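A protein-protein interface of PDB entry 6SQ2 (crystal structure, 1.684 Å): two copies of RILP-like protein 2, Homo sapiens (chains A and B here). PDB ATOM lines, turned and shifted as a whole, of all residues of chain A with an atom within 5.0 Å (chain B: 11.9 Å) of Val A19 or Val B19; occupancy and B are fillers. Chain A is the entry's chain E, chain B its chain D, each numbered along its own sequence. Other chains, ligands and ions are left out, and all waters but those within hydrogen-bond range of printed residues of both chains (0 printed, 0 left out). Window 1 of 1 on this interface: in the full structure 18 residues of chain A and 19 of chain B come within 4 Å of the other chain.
OE1 of Glu B22 lies within salt-bridge range of NH2 of Arg A23. The side-chain carboxylate (OE1) of Glu A22 is in salt-bridge range of the guanidinium group (NH1) of Arg B23 (2.8 Å).
OD1 of Asn B24 sits close to O of Leu B20, 3.4 Å away. NH1 of Arg A23 is in hydrogen-bond range of OD1 of Asn A24. The side-chain amide oxygen of Asn B24 sits at hydrogen-bond distance from the guanidinium group of Arg B23. O of Leu A20 lies close to ND2 of Asn A24 (3.2 Å).
Leu A16 touches Phe B11. Val B19 touches Val A19. Leu B20 touches Val A19. Val B19 touches Leu A20 (CG1 to CD2, 3.9 Å). Leu B26 touches Arg A23 (CD1 to O, 3.6 Å).
Of chain B, only Phe B11 comes within 4 Å of Leu A16. No residue of chain B comes within 4 Å of Asp A18. Of the printed residues of chain B, Val A19 touches Val B19 and Leu B20. Gln A21 touches none of the printed residues of chain B. Arg A23 touches just these residues of chain B: Glu B22 and Leu B26. Printed residues of chain A within 4 Å of Phe B11: Leu A16 (3.8 Å). Val B19 touches just these residues of chain A: Val A19 (3.5 Å) and Leu A20 (3.9 Å). Of the printed residues of chain A, Glu B22 touches Arg A23. Of the printed residues of chain A, Arg B23 touches Glu A22 (2.8 Å). Of the printed residues of chain A, Leu B26 touches Arg A23 (3.6 Å). The nearest printed residue of chain A that does not touch Arg B23 is Arg A23 (4.2 Å).
Of the 10 printed residues of chain A, 5 touch a printed residue of chain B. Printed residues of chain A that touch a printed residue of chain B: Leu A16, Val A19, Leu A20, Glu A22 and Arg A23. Hydrophobic or aromatic side chains of chain A that line the printed part of chain B: Leu A16, Val A19 and Leu A20. Of the 19 printed residues of chain B, 6 touch a printed residue of chain A. Hydrophobic or aromatic side chains of chain B within 4 Å of the printed part of chain A: Phe B11, Val B19, Leu B20 and Leu B26. Along chain B the printed residues that touch a printed residue of chain A span positions 11 to 26. Among the printed residues, Asp or Glu carboxylates within 4 Å of a Lys or Arg side-chain nitrogen of the other chain: Glu A22 with Arg B23 (2.8 Å) and Arg A23 with Glu B22 (2.9 Å).
Val B19 touches its own counterpart, Val A19. Val A19 touches Leu B20, and with the chains exchanged Leu A20 touches Val B19. Glu A22 touches Arg B23, and with the chains exchanged Arg A23 touches Glu B22.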
ATOM      1  N   GLU A  15      11.619  25.902   5.582  1.00  0.00           N
ATOM      2  CA  GLU A  15      11.833  24.518   6.004  1.00  0.00           C
ATOM      3  C   GLU A  15      11.780  24.393   7.524  1.00  0.00           C
ATOM      4  O   GLU A  15      11.100  23.513   8.063  1.00  0.00           O
ATOM      5  CB  GLU A  15      13.163  23.999   5.446  1.00  0.00           C
ATOM      6  CG  GLU A  15      13.084  23.610   3.959  1.00  0.00           C
ATOM      7  CD  GLU A  15      14.444  23.333   3.325  1.00  0.00           C
ATOM      8  OE1 GLU A  15      15.421  24.032   3.666  1.00  0.00           O
ATOM      9  OE2 GLU A  15      14.529  22.420   2.468  1.00  0.00           O
ATOM     10  N   LEU A  16      12.461  25.261   8.251  1.00  0.00           N
ATOM     11  CA  LEU A  16      12.417  25.196   9.699  1.00  0.00           C
ATOM     12  C   LEU A  16      11.037  25.558  10.261  1.00  0.00           C
ATOM     13  O   LEU A  16      10.570  24.946  11.139  1.00  0.00           O
ATOM     14  CB  LEU A  16      13.476  26.062  10.353  1.00  0.00           C
ATOM     15  CG  LEU A  16      13.562  25.931  11.860  1.00  0.00           C
ATOM     16  CD1 LEU A  16      14.115  24.634  12.313  1.00  0.00           C
ATOM     17  CD2 LEU A  16      14.375  27.036  12.463  1.00  0.00           C
ATOM     18  N   ARG A  17      10.429  26.576   9.714  1.00  0.00           N
ATOM     19  CA  ARG A  17       9.124  26.980  10.168  1.00  0.00           C
ATOM     20  C   ARG A  17       8.087  25.847  10.072  1.00  0.00           C
ATOM     21  O   ARG A  17       7.308  25.647  10.938  1.00  0.00           O
ATOM     22  CB  ARG A  17       8.699  28.208   9.434  1.00  0.00           C
ATOM     23  CG  ARG A  17       7.263  28.490   9.448  1.00  0.00           C
ATOM     24  CD  ARG A  17       6.927  29.951   9.285  1.00  0.00           C
ATOM     25  NE  ARG A  17       7.705  30.751   8.378  1.00  0.00           N
ATOM     26  CZ  ARG A  17       8.052  32.016   8.652  1.00  0.00           C
ATOM     27  NH1 ARG A  17       8.686  32.746   7.767  1.00  0.00           N
ATOM     28  NH2 ARG A  17       7.705  32.582   9.791  1.00  0.00           N
ATOM     29  N   ASP A  18       8.118  25.158   8.941  1.00  0.00           N
ATOM     30  CA  ASP A  18       7.197  24.089   8.677  1.00  0.00           C
ATOM     31  C   ASP A  18       7.332  22.961   9.713  1.00  0.00           C
ATOM     32  O   ASP A  18       6.380  22.486  10.234  1.00  0.00           O
ATOM     33  CB  ASP A  18       7.338  23.581   7.241  1.00  0.00           C
ATOM     34  CG  ASP A  18       6.695  24.490   6.209  1.00  0.00           C
ATOM     35  OD1 ASP A  18       6.154  25.508   6.586  1.00  0.00           O
ATOM     36  OD2 ASP A  18       6.694  24.144   5.002  1.00  0.00           O
ATOM     37  N   VAL A  19       8.535  22.567  10.014  1.00  0.00           N
ATOM     38  CA  VAL A  19       8.759  21.503  10.984  1.00  0.00           C
ATOM     39  C   VAL A  19       8.382  21.970  12.382  1.00  0.00           C
ATOM     40  O   VAL A  19       7.833  21.202  13.178  1.00  0.00           O
ATOM     41  CB  VAL A  19      10.216  21.013  10.933  1.00  0.00           C
ATOM     42  CG1 VAL A  19      10.397  19.832  11.857  1.00  0.00           C
ATOM     43  CG2 VAL A  19      10.592  20.615   9.518  1.00  0.00           C
ATOM     44  N   LEU A  20       8.670  23.235  12.705  1.00  0.00           N
ATOM     45  CA  LEU A  20       8.270  23.770  14.004  1.00  0.00           C
ATOM     46  C   LEU A  20       6.753  23.779  14.155  1.00  0.00           C
ATOM     47  O   LEU A  20       6.226  23.445  15.224  1.00  0.00           O
ATOM     48  CB  LEU A  20       8.835  25.179  14.196  1.00  0.00           C
ATOM     49  CG  LEU A  20      10.313  25.293  14.584  1.00  0.00           C
ATOM     50  CD1 LEU A  20      10.837  26.702  14.335  1.00  0.00           C
ATOM     51  CD2 LEU A  20      10.532  24.885  16.037  1.00  0.00           C
ATOM     52  N   GLN A  21       6.034  24.152  13.094  1.00  0.00           N
ATOM     53  CA  GLN A  21       4.577  24.163  13.156  1.00  0.00           C
ATOM     54  C   GLN A  21       4.016  22.759  13.341  1.00  0.00           C
ATOM     55  O   GLN A  21       3.063  22.566  14.104  1.00  0.00           O
ATOM     56  CB  GLN A  21       4.003  24.816  11.898  1.00  0.00           C
ATOM     57  CG  GLN A  21       4.198  26.321  11.858  1.00  0.00           C
ATOM     58  CD  GLN A  21       3.865  26.913  10.508  1.00  0.00           C
ATOM     59  OE1 GLN A  21       3.608  26.190   9.548  1.00  0.00           O
ATOM     60  NE2 GLN A  21       3.877  28.237  10.423  1.00  0.00           N
ATOM     61  N   GLU A  22       4.590  21.762  12.657  1.00  0.00           N
ATOM     62  CA  GLU A  22       4.118  20.395  12.864  1.00  0.00           C
ATOM     63  C   GLU A  22       4.430  19.919  14.277  1.00  0.00           C
ATOM     64  O   GLU A  22       3.590  19.283  14.923  1.00  0.00           O
ATOM     65  CB  GLU A  22       4.723  19.431  11.838  1.00  0.00           C
ATOM     66  CG  GLU A  22       4.073  18.045  11.937  1.00  0.00           C
ATOM     67  CD  GLU A  22       4.735  16.967  11.092  1.00  0.00           C
ATOM     68  OE1 GLU A  22       5.806  17.217  10.505  1.00  0.00           O
ATOM     69  OE2 GLU A  22       4.176  15.849  11.037  1.00  0.00           O
ATOM     70  N   ARG A  23       5.631  20.221  14.772  1.00  0.00           N
ATOM     71  CA  ARG A  23       5.967  19.884  16.151  1.00  0.00           C
ATOM     72  C   ARG A  23       4.970  20.504  17.121  1.00  0.00           C
ATOM     73  O   ARG A  23       4.492  19.833  18.047  1.00  0.00           O
ATOM     74  CB  ARG A  23       7.386  20.355  16.469  1.00  0.00           C
ATOM     75  CG  ARG A  23       7.957  19.776  17.748  1.00  0.00           C
ATOM     76  CD  ARG A  23       7.629  20.645  18.962  1.00  0.00           C
ATOM     77  NE  ARG A  23       7.504  22.064  18.638  1.00  0.00           N
ATOM     78  CZ  ARG A  23       8.474  22.954  18.821  1.00  0.00           C
ATOM     79  NH1 ARG A  23       8.282  24.228  18.511  1.00  0.00           N
ATOM     80  NH2 ARG A  23       9.644  22.566  19.312  1.00  0.00           N
ATOM     81  N   ASN A  24       4.638  21.783  16.918  1.00  0.00           N
ATOM     82  CA  ASN A  24       3.669  22.453  17.781  1.00  0.00           C
ATOM     83  C   ASN A  24       2.303  21.793  17.696  1.00  0.00           C
ATOM     84  O   ASN A  24       1.655  21.551  18.721  1.00  0.00           O
ATOM     85  CB  ASN A  24       3.558  23.929  17.402  1.00  0.00           C
ATOM     86  CG  ASN A  24       4.831  24.691  17.666  1.00  0.00           C
ATOM     87  OD1 ASN A  24       5.669  24.262  18.456  1.00  0.00           O
ATOM     88  ND2 ASN A  24       4.988  25.831  17.000  1.00  0.00           N
ATOM     89  N   PHE B  11      19.559  27.968   8.471  1.00  0.00           N
ATOM     90  CA  PHE B  11      19.653  27.117   9.629  1.00  0.00           C
ATOM     91  C   PHE B  11      20.551  25.921   9.435  1.00  0.00           C
ATOM     92  O   PHE B  11      20.679  25.453   8.361  1.00  0.00           O
ATOM     93  CB  PHE B  11      18.234  26.774  10.144  1.00  0.00           C
ATOM     94  CG  PHE B  11      17.406  27.974  10.353  1.00  0.00           C
ATOM     95  CD1 PHE B  11      17.681  28.795  11.412  1.00  0.00           C
ATOM     96  CD2 PHE B  11      16.453  28.341   9.486  1.00  0.00           C
ATOM     97  CE1 PHE B  11      16.993  29.914  11.595  1.00  0.00           C
ATOM     98  CE2 PHE B  11      15.725  29.473   9.680  1.00  0.00           C
ATOM     99  CZ  PHE B  11      16.006  30.271  10.741  1.00  0.00           C
ATOM    100  N   THR B  12      21.138  25.453  10.523  1.00  0.00           N
ATOM    101  CA  THR B  12      22.122  24.385  10.469  1.00  0.00           C
ATOM    102  C   THR B  12      21.454  23.014  10.465  1.00  0.00           C
ATOM    103  O   THR B  12      20.259  22.866  10.733  1.00  0.00           O
ATOM    104  CB  THR B  12      23.082  24.476  11.655  1.00  0.00           C
ATOM    105  OG1 THR B  12      22.371  24.178  12.861  1.00  0.00           O
ATOM    106  CG2 THR B  12      23.678  25.871  11.760  1.00  0.00           C
ATOM    107  N   LEU B  13      22.271  21.998  10.187  1.00  0.00           N
ATOM    108  CA  LEU B  13      21.796  20.621  10.232  1.00  0.00           C
ATOM    109  C   LEU B  13      21.320  20.247  11.632  1.00  0.00           C
ATOM    110  O   LEU B  13      20.244  19.664  11.801  1.00  0.00           O
ATOM    111  CB  LEU B  13      22.907  19.683   9.767  1.00  0.00           C
ATOM    112  CG  LEU B  13      22.676  18.183   9.927  1.00  0.00           C
ATOM    113  CD1 LEU B  13      21.487  17.735   9.093  1.00  0.00           C
ATOM    114  CD2 LEU B  13      23.935  17.427   9.536  1.00  0.00           C
ATOM    115  N   GLN B  14      22.113  20.575  12.656  1.00  0.00           N
ATOM    116  CA  GLN B  14      21.721  20.220  14.016  1.00  0.00           C
ATOM    117  C   GLN B  14      20.436  20.928  14.432  1.00  0.00           C
ATOM    118  O   GLN B  14      19.617  20.350  15.156  1.00  0.00           O
ATOM    119  CB  GLN B  14      22.856  20.537  14.993  1.00  0.00           C
ATOM    120  CG  GLN B  14      22.700  19.888  16.374  1.00  0.00           C
ATOM    121  CD  GLN B  14      22.851  18.371  16.344  1.00  0.00           C
ATOM    122  OE1 GLN B  14      23.700  17.830  15.634  1.00  0.00           O
ATOM    123  NE2 GLN B  14      22.024  17.678  17.125  1.00  0.00           N
ATOM    124  N   GLU B  15      20.226  22.160  13.964  1.00  0.00           N
ATOM    125  CA  GLU B  15      19.018  22.895  14.324  1.00  0.00           C
ATOM    126  C   GLU B  15      17.772  22.248  13.727  1.00  0.00           C
ATOM    127  O   GLU B  15      16.771  22.046  14.424  1.00  0.00           O
ATOM    128  CB  GLU B  15      19.140  24.350  13.874  1.00  0.00           C
ATOM    129  CG  GLU B  15      19.959  25.203  14.836  1.00  0.00           C
ATOM    130  CD  GLU B  15      20.612  26.399  14.173  1.00  0.00           C
ATOM    131  OE1 GLU B  15      20.299  26.692  12.996  1.00  0.00           O
ATOM    132  OE2 GLU B  15      21.446  27.056  14.836  1.00  0.00           O
ATOM    133  N   LEU B  16      17.802  21.937  12.431  1.00  0.00           N
ATOM    134  CA  LEU B  16      16.659  21.255  11.831  1.00  0.00           C
ATOM    135  C   LEU B  16      16.480  19.869  12.434  1.00  0.00           C
ATOM    136  O   LEU B  16      15.355  19.448  12.734  1.00  0.00           O
ATOM    137  CB  LEU B  16      16.830  21.163  10.313  1.00  0.00           C
ATOM    138  CG  LEU B  16      15.638  20.525   9.586  1.00  0.00           C
ATOM    139  CD1 LEU B  16      14.491  21.519   9.480  1.00  0.00           C
ATOM    140  CD2 LEU B  16      16.039  20.011   8.205  1.00  0.00           C
ATOM    141  N   ARG B  17      17.593  19.162  12.645  1.00  0.00           N
ATOM    142  CA  ARG B  17      17.555  17.796  13.155  1.00  0.00           C
ATOM    143  C   ARG B  17      16.895  17.720  14.519  1.00  0.00           C
ATOM    144  O   ARG B  17      16.106  16.805  14.784  1.00  0.00           O
ATOM    145  CB  ARG B  17      18.974  17.254  13.254  1.00  0.00           C
ATOM    146  CG  ARG B  17      19.372  16.331  12.154  1.00  0.00           C
ATOM    147  CD  ARG B  17      20.643  15.633  12.554  1.00  0.00           C
ATOM    148  NE  ARG B  17      20.798  14.382  11.834  1.00  0.00           N
ATOM    149  CZ  ARG B  17      21.961  13.915  11.412  1.00  0.00           C
ATOM    150  NH1 ARG B  17      22.009  12.764  10.756  1.00  0.00           N
ATOM    151  NH2 ARG B  17      23.072  14.597  11.658  1.00  0.00           N
ATOM    152  N   ASP B  18      17.235  18.647  15.417  1.00  0.00           N
ATOM    153  CA  ASP B  18      16.670  18.588  16.761  1.00  0.00           C
ATOM    154  C   ASP B  18      15.156  18.747  16.725  1.00  0.00           C
ATOM    155  O   ASP B  18      14.439  18.098  17.495  1.00  0.00           O
ATOM    156  CB  ASP B  18      17.307  19.651  17.653  1.00  0.00           C
ATOM    157  CG  ASP B  18      18.745  19.323  18.009  1.00  0.00           C
ATOM    158  OD1 ASP B  18      19.269  18.318  17.485  1.00  0.00           O
ATOM    159  OD2 ASP B  18      19.351  20.071  18.804  1.00  0.00           O
ATOM    160  N   VAL B  19      14.647  19.597  15.831  1.00  0.00           N
ATOM    161  CA  VAL B  19      13.200  19.742  15.720  1.00  0.00           C
ATOM    162  C   VAL B  19      12.591  18.497  15.090  1.00  0.00           C
ATOM    163  O   VAL B  19      11.528  18.031  15.516  1.00  0.00           O
ATOM    164  CB  VAL B  19      12.834  21.013  14.934  1.00  0.00           C
ATOM    165  CG1 VAL B  19      11.325  21.240  14.969  1.00  0.00           C
ATOM    166  CG2 VAL B  19      13.559  22.218  15.509  1.00  0.00           C
ATOM    167  N   LEU B  20      13.248  17.938  14.066  1.00  0.00           N
ATOM    168  CA  LEU B  20      12.735  16.720  13.441  1.00  0.00           C
ATOM    169  C   LEU B  20      12.674  15.573  14.438  1.00  0.00           C
ATOM    170  O   LEU B  20      11.711  14.796  14.447  1.00  0.00           O
ATOM    171  CB  LEU B  20      13.607  16.326  12.252  1.00  0.00           C
ATOM    172  CG  LEU B  20      13.384  17.066  10.939  1.00  0.00           C
ATOM    173  CD1 LEU B  20      14.477  16.665   9.958  1.00  0.00           C
ATOM    174  CD2 LEU B  20      12.001  16.766  10.369  1.00  0.00           C
ATOM    175  N   GLN B  21      13.734  15.538  15.214  1.00  0.00           N
ATOM    176  CA  GLN B  21      13.720  14.338  16.234  1.00  0.00           C
ATOM    177  C   GLN B  21      12.507  14.463  17.312  1.00  0.00           C
ATOM    178  O   GLN B  21      11.862  13.559  17.829  1.00  0.00           O
ATOM    179  CB  GLN B  21      15.097  14.243  16.897  1.00  0.00           C
ATOM    180  CG  GLN B  21      16.132  13.469  16.065  1.00  0.00           C
ATOM    181  CD  GLN B  21      17.571  13.929  16.298  1.00  0.00           C
ATOM    182  OE1 GLN B  21      17.869  14.615  17.278  1.00  0.00           O
ATOM    183  NE2 GLN B  21      18.470  13.542  15.394  1.00  0.00           N
ATOM    184  N   GLU B  22      12.334  15.737  17.680  1.00  0.00           N
ATOM    185  CA  GLU B  22      11.225  15.983  18.598  1.00  0.00           C
ATOM    186  C   GLU B  22       9.882  15.756  17.911  1.00  0.00           C
ATOM    187  O   GLU B  22       8.956  15.202  18.516  1.00  0.00           O
ATOM    188  CB  GLU B  22      11.311  17.401  19.155  1.00  0.00           C
ATOM    189  CG  GLU B  22      10.581  17.588  20.474  1.00  0.00           C
ATOM    190  CD  GLU B  22      10.042  18.994  20.655  1.00  0.00           C
ATOM    191  OE1 GLU B  22      10.668  19.946  20.140  1.00  0.00           O
ATOM    192  OE2 GLU B  22       9.001  19.150  21.331  1.00  0.00           O
ATOM    193  N   ARG B  23       9.757  16.184  16.652  1.00  0.00           N
ATOM    194  CA  ARG B  23       8.558  15.873  15.875  1.00  0.00           C
ATOM    195  C   ARG B  23       8.296  14.373  15.871  1.00  0.00           C
ATOM    196  O   ARG B  23       7.170  13.925  16.124  1.00  0.00           O
ATOM    197  CB  ARG B  23       8.709  16.396  14.443  1.00  0.00           C
ATOM    198  CG  ARG B  23       7.413  16.447  13.622  1.00  0.00           C
ATOM    199  CD  ARG B  23       7.053  15.096  13.003  1.00  0.00           C
ATOM    200  NE  ARG B  23       8.204  14.417  12.419  1.00  0.00           N
ATOM    201  CZ  ARG B  23       8.617  14.602  11.168  1.00  0.00           C
ATOM    202  NH1 ARG B  23       7.977  15.458  10.383  1.00  0.00           N
ATOM    203  NH2 ARG B  23       9.671  13.938  10.708  1.00  0.00           N
ATOM    204  N   ASN B  24       9.333  13.581  15.579  1.00  0.00           N
ATOM    205  CA  ASN B  24       9.183  12.127  15.527  1.00  0.00           C
ATOM    206  C   ASN B  24       8.757  11.564  16.878  1.00  0.00           C
ATOM    207  O   ASN B  24       7.869  10.707  16.950  1.00  0.00           O
ATOM    208  CB  ASN B  24      10.493  11.473  15.086  1.00  0.00           C
ATOM    209  CG  ASN B  24      10.840  11.756  13.637  1.00  0.00           C
ATOM    210  OD1 ASN B  24      10.020  12.266  12.870  1.00  0.00           O
ATOM    211  ND2 ASN B  24      12.068  11.422  13.251  1.00  0.00           N
ATOM    212  N   LYS B  25       9.400  12.015  17.956  1.00  0.00           N
ATOM    213  CA  LYS B  25       9.059  11.500  19.279  1.00  0.00           C
ATOM    214  C   LYS B  25       7.603  11.793  19.623  1.00  0.00           C
ATOM    215  O   LYS B  25       6.895  10.924  20.150  1.00  0.00           O
ATOM    216  CB  LYS B  25      10.002  12.094  20.329  1.00  0.00           C
ATOM    217  CG  LYS B  25       9.591  11.830  21.767  1.00  0.00           C
ATOM    218  CD  LYS B  25      10.776  11.969  22.712  1.00  0.00           C
ATOM    219  CE  LYS B  25      10.518  11.264  24.039  1.00  0.00           C
ATOM    220  NZ  LYS B  25      10.311   9.795  23.876  1.00  0.00           N
ATOM    221  N   LEU B  26       7.131  13.005  19.314  1.00  0.00           N
ATOM    222  CA  LEU B  26       5.742  13.356  19.591  1.00  0.00           C
ATOM    223  C   LEU B  26       4.783  12.529  18.743  1.00  0.00           C
ATOM    224  O   LEU B  26       3.739  12.082  19.233  1.00  0.00           O
ATOM    225  CB  LEU B  26       5.526  14.850  19.354  1.00  0.00           C
ATOM    226  CG  LEU B  26       6.205  15.773  20.368  1.00  0.00           C
ATOM    227  CD1 LEU B  26       6.218  17.202  19.861  1.00  0.00           C
ATOM    228  CD2 LEU B  26       5.493  15.688  21.718  1.00  0.00           C
ATOM    229  N   LYS B  27       5.123  12.314  17.470  1.00  0.00           N
ATOM    230  CA  LYS B  27       4.313  11.447  16.618  1.00  0.00           C
ATOM    231  C   LYS B  27       4.150  10.068  17.242  1.00  0.00           C
ATOM    232  O   LYS B  27       3.034   9.554  17.359  1.00  0.00           O
ATOM    233  CB  LYS B  27       4.954  11.330  15.235  1.00  0.00           C
ATOM    234  CG  LYS B  27       4.276  12.137  14.153  1.00  0.00           C
ATOM    235  CD  LYS B  27       4.613  11.584  12.771  1.00  0.00           C
ATOM    236  CE  LYS B  27       3.353  11.273  11.982  1.00  0.00           C
ATOM    237  NZ  LYS B  27       3.647  10.540  10.720  1.00  0.00           N
ATOM    238  N   SER B  28       5.262   9.452  17.652  1.00  0.00           N
ATOM    239  CA  SER B  28       5.204   8.122  18.248  1.00  0.00           C
ATOM    240  C   SER B  28       4.407   8.126  19.547  1.00  0.00           C
ATOM    241  O   SER B  28       3.637   7.194  19.812  1.00  0.00           O
ATOM    242  CB  SER B  28       6.618   7.597  18.492  1.00  0.00           C
ATOM    243  OG  SER B  28       7.309   7.432  17.262  1.00  0.00           O
ATOM    244  N   GLN B  29       4.581   9.165  20.372  1.00  0.00           N
ATOM    245  CA  GLN B  29       3.836   9.253  21.626  1.00  0.00           C
ATOM    246  C   GLN B  29       2.343   9.414  21.372  1.00  0.00           C
ATOM    247  O   GLN B  29       1.519   8.834  22.090  1.00  0.00           O
ATOM    248  CB  GLN B  29       4.359  10.416  22.472  1.00  0.00           C
ATOM    249  CG  GLN B  29       5.752  10.198  23.049  1.00  0.00           C
ATOM    250  CD  GLN B  29       6.261  11.396  23.832  1.00  0.00           C
ATOM    251  OE1 GLN B  29       5.861  12.534  23.584  1.00  0.00           O
ATOM    252  NE2 GLN B  29       7.153  11.143  24.782  1.00  0.00           N
